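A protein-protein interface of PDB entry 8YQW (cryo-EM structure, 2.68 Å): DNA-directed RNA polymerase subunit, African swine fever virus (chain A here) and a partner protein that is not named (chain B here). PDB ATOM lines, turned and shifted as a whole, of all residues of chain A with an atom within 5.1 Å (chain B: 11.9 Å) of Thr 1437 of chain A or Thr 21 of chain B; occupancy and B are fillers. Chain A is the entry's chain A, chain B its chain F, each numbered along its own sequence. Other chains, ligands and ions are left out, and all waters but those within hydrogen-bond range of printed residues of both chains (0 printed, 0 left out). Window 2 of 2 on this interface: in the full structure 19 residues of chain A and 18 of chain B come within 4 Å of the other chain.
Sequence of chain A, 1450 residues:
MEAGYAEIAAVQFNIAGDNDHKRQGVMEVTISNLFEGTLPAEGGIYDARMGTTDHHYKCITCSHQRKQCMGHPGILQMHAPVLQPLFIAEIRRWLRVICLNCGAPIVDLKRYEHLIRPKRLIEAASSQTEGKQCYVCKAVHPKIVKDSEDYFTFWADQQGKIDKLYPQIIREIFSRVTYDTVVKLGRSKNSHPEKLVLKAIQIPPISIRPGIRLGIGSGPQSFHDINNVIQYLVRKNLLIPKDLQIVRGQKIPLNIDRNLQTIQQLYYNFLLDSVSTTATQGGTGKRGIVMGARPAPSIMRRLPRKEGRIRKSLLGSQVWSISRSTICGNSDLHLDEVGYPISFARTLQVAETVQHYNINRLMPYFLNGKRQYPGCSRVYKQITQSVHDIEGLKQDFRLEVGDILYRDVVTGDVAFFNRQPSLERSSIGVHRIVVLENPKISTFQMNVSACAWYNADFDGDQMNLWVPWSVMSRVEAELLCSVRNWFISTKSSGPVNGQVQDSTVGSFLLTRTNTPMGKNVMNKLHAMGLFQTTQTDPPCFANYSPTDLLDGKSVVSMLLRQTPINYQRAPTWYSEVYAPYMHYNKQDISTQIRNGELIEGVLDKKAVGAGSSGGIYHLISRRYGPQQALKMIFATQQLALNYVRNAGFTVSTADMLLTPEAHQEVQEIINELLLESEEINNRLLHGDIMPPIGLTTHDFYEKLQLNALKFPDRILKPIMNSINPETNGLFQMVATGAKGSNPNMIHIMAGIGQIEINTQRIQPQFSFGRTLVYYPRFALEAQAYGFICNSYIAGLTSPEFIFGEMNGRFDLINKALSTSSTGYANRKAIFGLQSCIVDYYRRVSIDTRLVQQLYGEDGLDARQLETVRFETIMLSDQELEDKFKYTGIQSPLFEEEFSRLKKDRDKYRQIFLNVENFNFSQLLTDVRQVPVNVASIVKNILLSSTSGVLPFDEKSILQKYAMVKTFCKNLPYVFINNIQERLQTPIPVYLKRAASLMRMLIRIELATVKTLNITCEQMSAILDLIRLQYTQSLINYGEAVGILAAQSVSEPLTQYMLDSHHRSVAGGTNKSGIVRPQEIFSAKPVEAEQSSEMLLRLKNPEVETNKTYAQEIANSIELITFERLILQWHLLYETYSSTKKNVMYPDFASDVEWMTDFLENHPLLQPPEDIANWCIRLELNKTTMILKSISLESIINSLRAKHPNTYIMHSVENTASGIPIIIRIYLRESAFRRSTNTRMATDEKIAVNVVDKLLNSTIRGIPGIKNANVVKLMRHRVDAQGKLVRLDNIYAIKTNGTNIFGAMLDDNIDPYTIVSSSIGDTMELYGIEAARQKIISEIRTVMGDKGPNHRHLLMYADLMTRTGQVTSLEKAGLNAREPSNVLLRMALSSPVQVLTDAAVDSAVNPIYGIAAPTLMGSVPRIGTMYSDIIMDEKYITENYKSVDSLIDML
Of the 10 printed residues of chain A, 6 touch a printed residue of chain B. Printed residues of chain B that touch a printed residue of chain A: Thr 17, Asn 18, Cys 20, Thr 21 and Val 23. Among the printed residues, 11 pairs touch across the chains.
OG1 of Thr 21 of chain B sits at hydrogen-bond distance from O of Asn 18 of chain B, at 2.4 Å. The backbone carbonyl oxygen (O) of Pro 16 of chain B lies within hydrogen-bond range of the side-chain sulfur (SG) of Cys 20 of chain B. The backbone carbonyl oxygen of Lys 1434 of chain A lies within hydrogen-bond range of the side-chain hydroxyl of Thr 1437 of chain A (2.8 Å).
Lys 1434 of chain A touches none of the printed residues of chain B. Of chain B, only Cys 20 (3.3 Å) and Thr 21 (3.3 Å) come within 4 Å of Thr 1437 of chain A. No residue of chain B comes within 4 Å of Glu 1438 of chain A. Of chain B, only Thr 21 (3.97 Å) comes within 4 Å of Lys 1441 of chain A. Asp 14 of chain B touches none of the printed residues of chain A. Printed residues of chain A within 4 Å of Thr 17 of chain B: Ile 1436 (3.5 Å) and Tyr 1440 (3.8 Å). Of the printed residues of chain A, Asn 18 of chain B touches Ser 1442. Printed residues of chain A within 4 Å of Cys 20 of chain B: Glu 1433 (3.9 Å), Ile 1436 (3.8 Å) and Thr 1437 (3.3 Å). Thr 21 of chain B touches just these residues of chain A: Ile 1436, Thr 1437, Lys 1441 and Ser 1442. Of the printed residues of chain A, Val 23 of chain B touches Glu 1433. Pro 56 of chain B touches none of the printed residues of chain A.
The side-chain hydroxyl of Ser 1442 of chain A sits at hydrogen-bond distance from the side-chain hydroxyl of Thr 21 of chain B, at 3.0 Å.
Glu 1433 of chain A touches Cys 20 of chain B (OE2 to O, 3.9 Å). Val 23 of chain B touches Glu 1433 of chain A (CG2 to CG, 3.5 Å). Ile 1436 of chain A touches Thr 17 of chain B. Ile 1436 of chain A touches Cys 20 of chain B. CG2 of Ile 1436 of chain A touches CG2 of Thr 21 of chain B, 3.7 Å away. Thr 1437 of chain A touches Cys 20 of chain B. Thr 1437 of chain A touches Thr 21 of chain B. Thr 17 of chain B touches Tyr 1440 of chain A. CG2 of Thr 21 of chain B touches C of Lys 1441 of chain A, 3.97 Å away. Asn 18 of chain B touches Ser 1442 of chain A (OD1 to CA, 3.4 Å).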
ATOM      1  N   GLU A1433      36.899   3.056  24.780  1.00  0.00           N
ATOM      2  CA  GLU A1433      35.736   3.740  25.334  1.00  0.00           C
ATOM      3  C   GLU A1433      35.645   5.178  24.834  1.00  0.00           C
ATOM      4  O   GLU A1433      34.565   5.650  24.470  1.00  0.00           O
ATOM      5  CB  GLU A1433      35.796   3.698  26.861  1.00  0.00           C
ATOM      6  CG  GLU A1433      34.492   4.022  27.561  1.00  0.00           C
ATOM      7  CD  GLU A1433      34.321   5.499  27.854  1.00  0.00           C
ATOM      8  OE1 GLU A1433      35.340   6.205  27.988  1.00  0.00           O
ATOM      9  OE2 GLU A1433      33.163   5.953  27.956  1.00  0.00           O
ATOM     10  N   LYS A1434      36.775   5.887  24.804  1.00  0.00           N
ATOM     11  CA  LYS A1434      36.747   7.303  24.451  1.00  0.00           C
ATOM     12  C   LYS A1434      36.502   7.506  22.962  1.00  0.00           C
ATOM     13  O   LYS A1434      35.764   8.415  22.568  1.00  0.00           O
ATOM     14  CB  LYS A1434      38.053   7.971  24.875  1.00  0.00           C
ATOM     15  CG  LYS A1434      38.248   9.371  24.322  1.00  0.00           C
ATOM     16  CD  LYS A1434      39.163  10.193  25.214  1.00  0.00           C
ATOM     17  CE  LYS A1434      40.548   9.576  25.293  1.00  0.00           C
ATOM     18  NZ  LYS A1434      41.212   9.541  23.965  1.00  0.00           N
ATOM     19  N   TYR A1435      37.115   6.673  22.120  1.00  0.00           N
ATOM     20  CA  TYR A1435      36.951   6.814  20.677  1.00  0.00           C
ATOM     21  C   TYR A1435      35.506   6.584  20.258  1.00  0.00           C
ATOM     22  O   TYR A1435      34.996   7.264  19.360  1.00  0.00           O
ATOM     23  CB  TYR A1435      37.881   5.841  19.955  1.00  0.00           C
ATOM     24  CG  TYR A1435      37.947   6.022  18.458  1.00  0.00           C
ATOM     25  CD1 TYR A1435      38.610   7.103  17.901  1.00  0.00           C
ATOM     26  CD2 TYR A1435      37.362   5.103  17.603  1.00  0.00           C
ATOM     27  CE1 TYR A1435      38.679   7.266  16.536  1.00  0.00           C
ATOM     28  CE2 TYR A1435      37.427   5.260  16.237  1.00  0.00           C
ATOM     29  CZ  TYR A1435      38.086   6.344  15.709  1.00  0.00           C
ATOM     30  OH  TYR A1435      38.154   6.506  14.348  1.00  0.00           O
ATOM     31  N   ILE A1436      34.834   5.623  20.891  1.00  0.00           N
ATOM     32  CA  ILE A1436      33.478   5.264  20.487  1.00  0.00           C
ATOM     33  C   ILE A1436      32.493   6.371  20.843  1.00  0.00           C
ATOM     34  O   ILE A1436      31.581   6.680  20.068  1.00  0.00           O
ATOM     35  CB  ILE A1436      33.085   3.920  21.120  1.00  0.00           C
ATOM     36  CG1 ILE A1436      33.874   2.787  20.471  1.00  0.00           C
ATOM     37  CG2 ILE A1436      31.602   3.668  20.970  1.00  0.00           C
ATOM     38  CD1 ILE A1436      33.689   1.460  21.152  1.00  0.00           C
ATOM     39  N   THR A1437      32.658   6.990  22.015  1.00  0.00           N
ATOM     40  CA  THR A1437      31.732   8.039  22.430  1.00  0.00           C
ATOM     41  C   THR A1437      31.756   9.216  21.464  1.00  0.00           C
ATOM     42  O   THR A1437      30.711   9.801  21.159  1.00  0.00           O
ATOM     43  CB  THR A1437      32.060   8.512  23.845  1.00  0.00           C
ATOM     44  OG1 THR A1437      33.397   9.023  23.880  1.00  0.00           O
ATOM     45  CG2 THR A1437      31.931   7.372  24.833  1.00  0.00           C
ATOM     46  N   GLU A1438      32.940   9.584  20.977  1.00  0.00           N
ATOM     47  CA  GLU A1438      33.051  10.727  20.079  1.00  0.00           C
ATOM     48  C   GLU A1438      32.583  10.404  18.666  1.00  0.00           C
ATOM     49  O   GLU A1438      32.036  11.279  17.987  1.00  0.00           O
ATOM     50  CB  GLU A1438      34.495  11.229  20.047  1.00  0.00           C
ATOM     51  CG  GLU A1438      34.630  12.719  19.771  1.00  0.00           C
ATOM     52  CD  GLU A1438      34.438  13.070  18.307  1.00  0.00           C
ATOM     53  OE1 GLU A1438      34.738  12.218  17.446  1.00  0.00           O
ATOM     54  OE2 GLU A1438      33.982  14.196  18.018  1.00  0.00           O
ATOM     55  N   ASN A1439      32.775   9.170  18.211  1.00  0.00           N
ATOM     56  CA  ASN A1439      32.568   8.825  16.811  1.00  0.00           C
ATOM     57  C   ASN A1439      31.325   7.990  16.547  1.00  0.00           C
ATOM     58  O   ASN A1439      30.826   7.998  15.422  1.00  0.00           O
ATOM     59  CB  ASN A1439      33.790   8.073  16.272  1.00  0.00           C
ATOM     60  CG  ASN A1439      34.960   8.992  15.997  1.00  0.00           C
ATOM     61  OD1 ASN A1439      34.925   9.798  15.069  1.00  0.00           O
ATOM     62  ND2 ASN A1439      35.995   8.890  16.817  1.00  0.00           N
ATOM     63  N   TYR A1440      30.814   7.273  17.542  1.00  0.00           N
ATOM     64  CA  TYR A1440      29.689   6.370  17.351  1.00  0.00           C
ATOM     65  C   TYR A1440      28.459   6.889  18.085  1.00  0.00           C
ATOM     66  O   TYR A1440      28.533   7.791  18.925  1.00  0.00           O
ATOM     67  CB  TYR A1440      30.031   4.955  17.835  1.00  0.00           C
ATOM     68  CG  TYR A1440      31.011   4.203  16.962  1.00  0.00           C
ATOM     69  CD1 TYR A1440      32.291   4.687  16.735  1.00  0.00           C
ATOM     70  CD2 TYR A1440      30.659   2.997  16.377  1.00  0.00           C
ATOM     71  CE1 TYR A1440      33.186   3.998  15.945  1.00  0.00           C
ATOM     72  CE2 TYR A1440      31.548   2.302  15.585  1.00  0.00           C
ATOM     73  CZ  TYR A1440      32.809   2.806  15.373  1.00  0.00           C
ATOM     74  OH  TYR A1440      33.699   2.116  14.583  1.00  0.00           O
ATOM     75  N   LYS A1441      27.315   6.294  17.756  1.00  0.00           N
ATOM     76  CA  LYS A1441      26.040   6.645  18.359  1.00  0.00           C
ATOM     77  C   LYS A1441      25.314   5.379  18.789  1.00  0.00           C
ATOM     78  O   LYS A1441      25.540   4.298  18.239  1.00  0.00           O
ATOM     79  CB  LYS A1441      25.157   7.446  17.389  1.00  0.00           C
ATOM     80  CG  LYS A1441      25.774   8.747  16.906  1.00  0.00           C
ATOM     81  CD  LYS A1441      26.051   9.694  18.062  1.00  0.00           C
ATOM     82  CE  LYS A1441      26.340  11.101  17.565  1.00  0.00           C
ATOM     83  NZ  LYS A1441      27.556  11.152  16.710  1.00  0.00           N
ATOM     84  N   SER A1442      24.442   5.524  19.781  1.00  0.00           N
ATOM     85  CA  SER A1442      23.673   4.398  20.295  1.00  0.00           C
ATOM     86  C   SER A1442      22.615   3.959  19.289  1.00  0.00           C
ATOM     87  O   SER A1442      22.046   2.873  19.404  1.00  0.00           O
ATOM     88  CB  SER A1442      23.013   4.760  21.627  1.00  0.00           C
ATOM     89  OG  SER A1442      23.984   5.048  22.619  1.00  0.00           O
ATOM     90  N   ILE B  13      28.687  -8.408  28.416  1.00  0.00           N
ATOM     91  CA  ILE B  13      28.233  -7.357  27.518  1.00  0.00           C
ATOM     92  C   ILE B  13      28.100  -7.972  26.134  1.00  0.00           C
ATOM     93  O   ILE B  13      29.099  -8.390  25.537  1.00  0.00           O
ATOM     94  CB  ILE B  13      29.193  -6.164  27.503  1.00  0.00           C
ATOM     95  CG1 ILE B  13      29.218  -5.498  28.880  1.00  0.00           C
ATOM     96  CG2 ILE B  13      28.791  -5.177  26.435  1.00  0.00           C
ATOM     97  CD1 ILE B  13      30.542  -4.888  29.241  1.00  0.00           C
ATOM     98  N   ASP B  14      26.870  -8.032  25.623  1.00  0.00           N
ATOM     99  CA  ASP B  14      26.621  -8.693  24.349  1.00  0.00           C
ATOM    100  C   ASP B  14      27.013  -7.829  23.158  1.00  0.00           C
ATOM    101  O   ASP B  14      27.444  -8.363  22.131  1.00  0.00           O
ATOM    102  CB  ASP B  14      25.149  -9.091  24.249  1.00  0.00           C
ATOM    103  CG  ASP B  14      24.779 -10.185  25.227  1.00  0.00           C
ATOM    104  OD1 ASP B  14      25.674 -10.956  25.630  1.00  0.00           O
ATOM    105  OD2 ASP B  14      23.589 -10.278  25.593  1.00  0.00           O
ATOM    106  N   ASP B  15      26.876  -6.510  23.267  1.00  0.00           N
ATOM    107  CA  ASP B  15      27.221  -5.589  22.187  1.00  0.00           C
ATOM    108  C   ASP B  15      28.199  -4.560  22.733  1.00  0.00           C
ATOM    109  O   ASP B  15      27.796  -3.474  23.172  1.00  0.00           O
ATOM    110  CB  ASP B  15      25.978  -4.921  21.608  1.00  0.00           C
ATOM    111  CG  ASP B  15      26.255  -4.216  20.300  1.00  0.00           C
ATOM    112  OD1 ASP B  15      27.348  -4.419  19.735  1.00  0.00           O
ATOM    113  OD2 ASP B  15      25.374  -3.467  19.830  1.00  0.00           O
ATOM    114  N   PRO B  16      29.496  -4.871  22.729  1.00  0.00           N
ATOM    115  CA  PRO B  16      30.475  -3.936  23.304  1.00  0.00           C
ATOM    116  C   PRO B  16      30.525  -2.589  22.606  1.00  0.00           C
ATOM    117  O   PRO B  16      30.839  -1.582  23.250  1.00  0.00           O
ATOM    118  CB  PRO B  16      31.799  -4.699  23.164  1.00  0.00           C
ATOM    119  CG  PRO B  16      31.408  -6.126  23.025  1.00  0.00           C
ATOM    120  CD  PRO B  16      30.132  -6.111  22.263  1.00  0.00           C
ATOM    121  N   THR B  17      30.233  -2.537  21.305  1.00  0.00           N
ATOM    122  CA  THR B  17      30.289  -1.270  20.584  1.00  0.00           C
ATOM    123  C   THR B  17      29.203  -0.313  21.060  1.00  0.00           C
ATOM    124  O   THR B  17      29.466   0.867  21.312  1.00  0.00           O
ATOM    125  CB  THR B  17      30.160  -1.516  19.083  1.00  0.00           C
ATOM    126  OG1 THR B  17      31.029  -2.587  18.696  1.00  0.00           O
ATOM    127  CG2 THR B  17      30.540  -0.263  18.312  1.00  0.00           C
ATOM    128  N   ASN B  18      27.968  -0.806  21.179  1.00  0.00           N
ATOM    129  CA  ASN B  18      26.873   0.033  21.650  1.00  0.00           C
ATOM    130  C   ASN B  18      26.996   0.332  23.137  1.00  0.00           C
ATOM    131  O   ASN B  18      26.603   1.415  23.584  1.00  0.00           O
ATOM    132  CB  ASN B  18      25.536  -0.644  21.352  1.00  0.00           C
ATOM    133  CG  ASN B  18      24.350   0.248  21.647  1.00  0.00           C
ATOM    134  OD1 ASN B  18      24.491   1.457  21.820  1.00  0.00           O
ATOM    135  ND2 ASN B  18      23.166  -0.347  21.703  1.00  0.00           N
ATOM    136  N   PHE B  19      27.531  -0.612  23.912  1.00  0.00           N
ATOM    137  CA  PHE B  19      27.651  -0.418  25.353  1.00  0.00           C
ATOM    138  C   PHE B  19      28.574   0.747  25.684  1.00  0.00           C
ATOM    139  O   PHE B  19      28.293   1.529  26.599  1.00  0.00           O
ATOM    140  CB  PHE B  19      28.155  -1.704  26.004  1.00  0.00           C
ATOM    141  CG  PHE B  19      28.200  -1.653  27.502  1.00  0.00           C
ATOM    142  CD1 PHE B  19      27.082  -1.972  28.252  1.00  0.00           C
ATOM    143  CD2 PHE B  19      29.362  -1.300  28.162  1.00  0.00           C
ATOM    144  CE1 PHE B  19      27.123  -1.928  29.628  1.00  0.00           C
ATOM    145  CE2 PHE B  19      29.405  -1.254  29.536  1.00  0.00           C
ATOM    146  CZ  PHE B  19      28.286  -1.570  30.270  1.00  0.00           C
ATOM    147  N   CYS B  20      29.677   0.879  24.952  1.00  0.00           N
ATOM    148  CA  CYS B  20      30.700   1.863  25.283  1.00  0.00           C
ATOM    149  C   CYS B  20      30.325   3.285  24.890  1.00  0.00           C
ATOM    150  O   CYS B  20      31.063   4.213  25.233  1.00  0.00           O
ATOM    151  CB  CYS B  20      32.024   1.481  24.622  1.00  0.00           C
ATOM    152  SG  CYS B  20      32.817   0.046  25.368  1.00  0.00           S
ATOM    153  N   THR B  21      29.212   3.480  24.180  1.00  0.00           N
ATOM    154  CA  THR B  21      28.778   4.836  23.858  1.00  0.00           C
ATOM    155  C   THR B  21      28.418   5.611  25.118  1.00  0.00           C
ATOM    156  O   THR B  21      28.730   6.802  25.235  1.00  0.00           O
ATOM    157  CB  THR B  21      27.592   4.796  22.897  1.00  0.00           C
ATOM    158  OG1 THR B  21      26.642   3.828  23.349  1.00  0.00           O
ATOM    159  CG2 THR B  21      28.055   4.424  21.502  1.00  0.00           C
ATOM    160  N   ASN B  22      27.758   4.954  26.073  1.00  0.00           N
ATOM    161  CA  ASN B  22      27.426   5.550  27.371  1.00  0.00           C
ATOM    162  C   ASN B  22      27.657   4.470  28.427  1.00  0.00           C
ATOM    163  O   ASN B  22      26.755   3.689  28.735  1.00  0.00           O
ATOM    164  CB  ASN B  22      25.996   6.071  27.388  1.00  0.00           C
ATOM    165  CG  ASN B  22      25.786   7.162  28.413  1.00  0.00           C
ATOM    166  OD1 ASN B  22      26.714   7.558  29.117  1.00  0.00           O
ATOM    167  ND2 ASN B  22      24.561   7.664  28.498  1.00  0.00           N
ATOM    168  N   VAL B  23      28.874   4.432  28.975  1.00  0.00           N
ATOM    169  CA  VAL B  23      29.245   3.335  29.862  1.00  0.00           C
ATOM    170  C   VAL B  23      28.575   3.477  31.222  1.00  0.00           C
ATOM    171  O   VAL B  23      28.121   2.488  31.802  1.00  0.00           O
ATOM    172  CB  VAL B  23      30.774   3.240  29.992  1.00  0.00           C
ATOM    173  CG1 VAL B  23      31.150   2.248  31.071  1.00  0.00           C
ATOM    174  CG2 VAL B  23      31.374   2.812  28.679  1.00  0.00           C
ATOM    175  N   GLU B  24      28.507   4.693  31.761  1.00  0.00           N
ATOM    176  CA  GLU B  24      27.951   4.854  33.102  1.00  0.00           C
ATOM    177  C   GLU B  24      26.452   4.573  33.124  1.00  0.00           C
ATOM    178  O   GLU B  24      25.963   3.852  34.004  1.00  0.00           O
ATOM    179  CB  GLU B  24      28.270   6.252  33.640  1.00  0.00           C
ATOM    180  CG  GLU B  24      27.722   7.413  32.821  1.00  0.00           C
ATOM    181  CD  GLU B  24      26.410   7.950  33.366  1.00  0.00           C
ATOM    182  OE1 GLU B  24      26.133   7.744  34.566  1.00  0.00           O
ATOM    183  OE2 GLU B  24      25.655   8.577  32.592  1.00  0.00           O
ATOM    184  N   ALA B  25      25.710   5.098  32.145  1.00  0.00           N
ATOM    185  CA  ALA B  25      24.270   4.872  32.106  1.00  0.00           C
ATOM    186  C   ALA B  25      23.948   3.407  31.847  1.00  0.00           C
ATOM    187  O   ALA B  25      23.096   2.820  32.523  1.00  0.00           O
ATOM    188  CB  ALA B  25      23.628   5.762  31.044  1.00  0.00           C
ATOM    189  N   HIS B  26      24.623   2.798  30.869  1.00  0.00           N
ATOM    190  CA  HIS B  26      24.388   1.389  30.575  1.00  0.00           C
ATOM    191  C   HIS B  26      24.778   0.509  31.753  1.00  0.00           C
ATOM    192  O   HIS B  26      24.100  -0.478  32.053  1.00  0.00           O
ATOM    193  CB  HIS B  26      25.157   0.977  29.322  1.00  0.00           C
ATOM    194  CG  HIS B  26      24.581   1.516  28.050  1.00  0.00           C
ATOM    195  ND1 HIS B  26      25.136   2.579  27.373  1.00  0.00           N
ATOM    196  CD2 HIS B  26      23.500   1.136  27.330  1.00  0.00           C
ATOM    197  CE1 HIS B  26      24.422   2.833  26.292  1.00  0.00           C
ATOM    198  NE2 HIS B  26      23.423   1.971  26.243  1.00  0.00           N
ATOM    199  N   LEU B  27      25.875   0.850  32.429  1.00  0.00           N
ATOM    200  CA  LEU B  27      26.322   0.080  33.583  1.00  0.00           C
ATOM    201  C   LEU B  27      25.299   0.135  34.708  1.00  0.00           C
ATOM    202  O   LEU B  27      24.946  -0.897  35.290  1.00  0.00           O
ATOM    203  CB  LEU B  27      27.676   0.607  34.057  1.00  0.00           C
ATOM    204  CG  LEU B  27      28.604  -0.360  34.781  1.00  0.00           C
ATOM    205  CD1 LEU B  27      28.919  -1.541  33.894  1.00  0.00           C
ATOM    206  CD2 LEU B  27      29.874   0.354  35.187  1.00  0.00           C
ATOM    207  N   LEU B  28      24.806   1.334  35.026  1.00  0.00           N
ATOM    208  CA  LEU B  28      23.783   1.449  36.060  1.00  0.00           C
ATOM    209  C   LEU B  28      22.514   0.709  35.661  1.00  0.00           C
ATOM    210  O   LEU B  28      21.891   0.038  36.491  1.00  0.00           O
ATOM    211  CB  LEU B  28      23.478   2.918  36.345  1.00  0.00           C
ATOM    212  CG  LEU B  28      24.465   3.651  37.248  1.00  0.00           C
ATOM    213  CD1 LEU B  28      24.117   5.126  37.323  1.00  0.00           C
ATOM    214  CD2 LEU B  28      24.469   3.032  38.633  1.00  0.00           C
ATOM    215  N   LYS B  29      22.119   0.816  34.392  1.00  0.00           N
ATOM    216  CA  LYS B  29      20.916   0.142  33.921  1.00  0.00           C
ATOM    217  C   LYS B  29      21.036  -1.371  34.064  1.00  0.00           C
ATOM    218  O   LYS B  29      20.115  -2.033  34.558  1.00  0.00           O
ATOM    219  CB  LYS B  29      20.666   0.530  32.465  1.00  0.00           C
ATOM    220  CG  LYS B  29      19.327   0.130  31.897  1.00  0.00           C
ATOM    221  CD  LYS B  29      19.300   0.429  30.408  1.00  0.00           C
ATOM    222  CE  LYS B  29      19.364   1.927  30.148  1.00  0.00           C
ATOM    223  NZ  LYS B  29      19.283   2.249  28.698  1.00  0.00           N
ATOM    224  N   ARG B  54      35.389   0.663  38.077  1.00  0.00           N
ATOM    225  CA  ARG B  54      35.088  -0.426  37.162  1.00  0.00           C
ATOM    226  C   ARG B  54      36.373  -0.827  36.451  1.00  0.00           C
ATOM    227  O   ARG B  54      37.467  -0.374  36.796  1.00  0.00           O
ATOM    228  CB  ARG B  54      33.994  -0.010  36.169  1.00  0.00           C
ATOM    229  CG  ARG B  54      34.466   1.009  35.154  1.00  0.00           C
ATOM    230  CD  ARG B  54      33.412   1.297  34.114  1.00  0.00           C
ATOM    231  NE  ARG B  54      33.983   1.972  32.955  1.00  0.00           N
ATOM    232  CZ  ARG B  54      34.014   3.286  32.790  1.00  0.00           C
ATOM    233  NH1 ARG B  54      33.502   4.108  33.690  1.00  0.00           N
ATOM    234  NH2 ARG B  54      34.568   3.788  31.691  1.00  0.00           N
ATOM    235  N   PRO B  56      38.152  -1.713  32.336  1.00  0.00           N
ATOM    236  CA  PRO B  56      37.901  -1.556  30.903  1.00  0.00           C
ATOM    237  C   PRO B  56      37.021  -2.685  30.395  1.00  0.00           C
ATOM    238  O   PRO B  56      36.904  -3.739  31.021  1.00  0.00           O
ATOM    239  CB  PRO B  56      39.301  -1.618  30.286  1.00  0.00           C
ATOM    240  CG  PRO B  56      40.217  -1.248  31.382  1.00  0.00           C
ATOM    241  CD  PRO B  56      39.592  -1.747  32.644  1.00  0.00           C
ATOM    242  N   CYS B  57      36.387  -2.454  29.251  1.00  0.00           N
ATOM    243  CA  CYS B  57      35.582  -3.508  28.650  1.00  0.00           C
ATOM    244  C   CYS B  57      36.482  -4.487  27.910  1.00  0.00           C
ATOM    245  O   CYS B  57      36.816  -4.269  26.743  1.00  0.00           O
ATOM    246  CB  CYS B  57      34.532  -2.922  27.707  1.00  0.00           C
ATOM    247  SG  CYS B  57      33.413  -4.142  26.988  1.00  0.00           S
ATOM    248  N   MET B  70      33.047  -6.945  31.999  1.00  0.00           N
ATOM    249  CA  MET B  70      33.530  -5.808  32.768  1.00  0.00           C
ATOM    250  C   MET B  70      33.375  -6.084  34.254  1.00  0.00           C
ATOM    251  O   MET B  70      32.297  -6.478  34.702  1.00  0.00           O
ATOM    252  CB  MET B  70      32.776  -4.532  32.384  1.00  0.00           C
ATOM    253  CG  MET B  70      33.428  -3.261  32.865  1.00  0.00           C
ATOM    254  SD  MET B  70      32.321  -1.851  32.772  1.00  0.00           S
ATOM    255  CE  MET B  70      32.641  -1.303  31.102  1.00  0.00           C
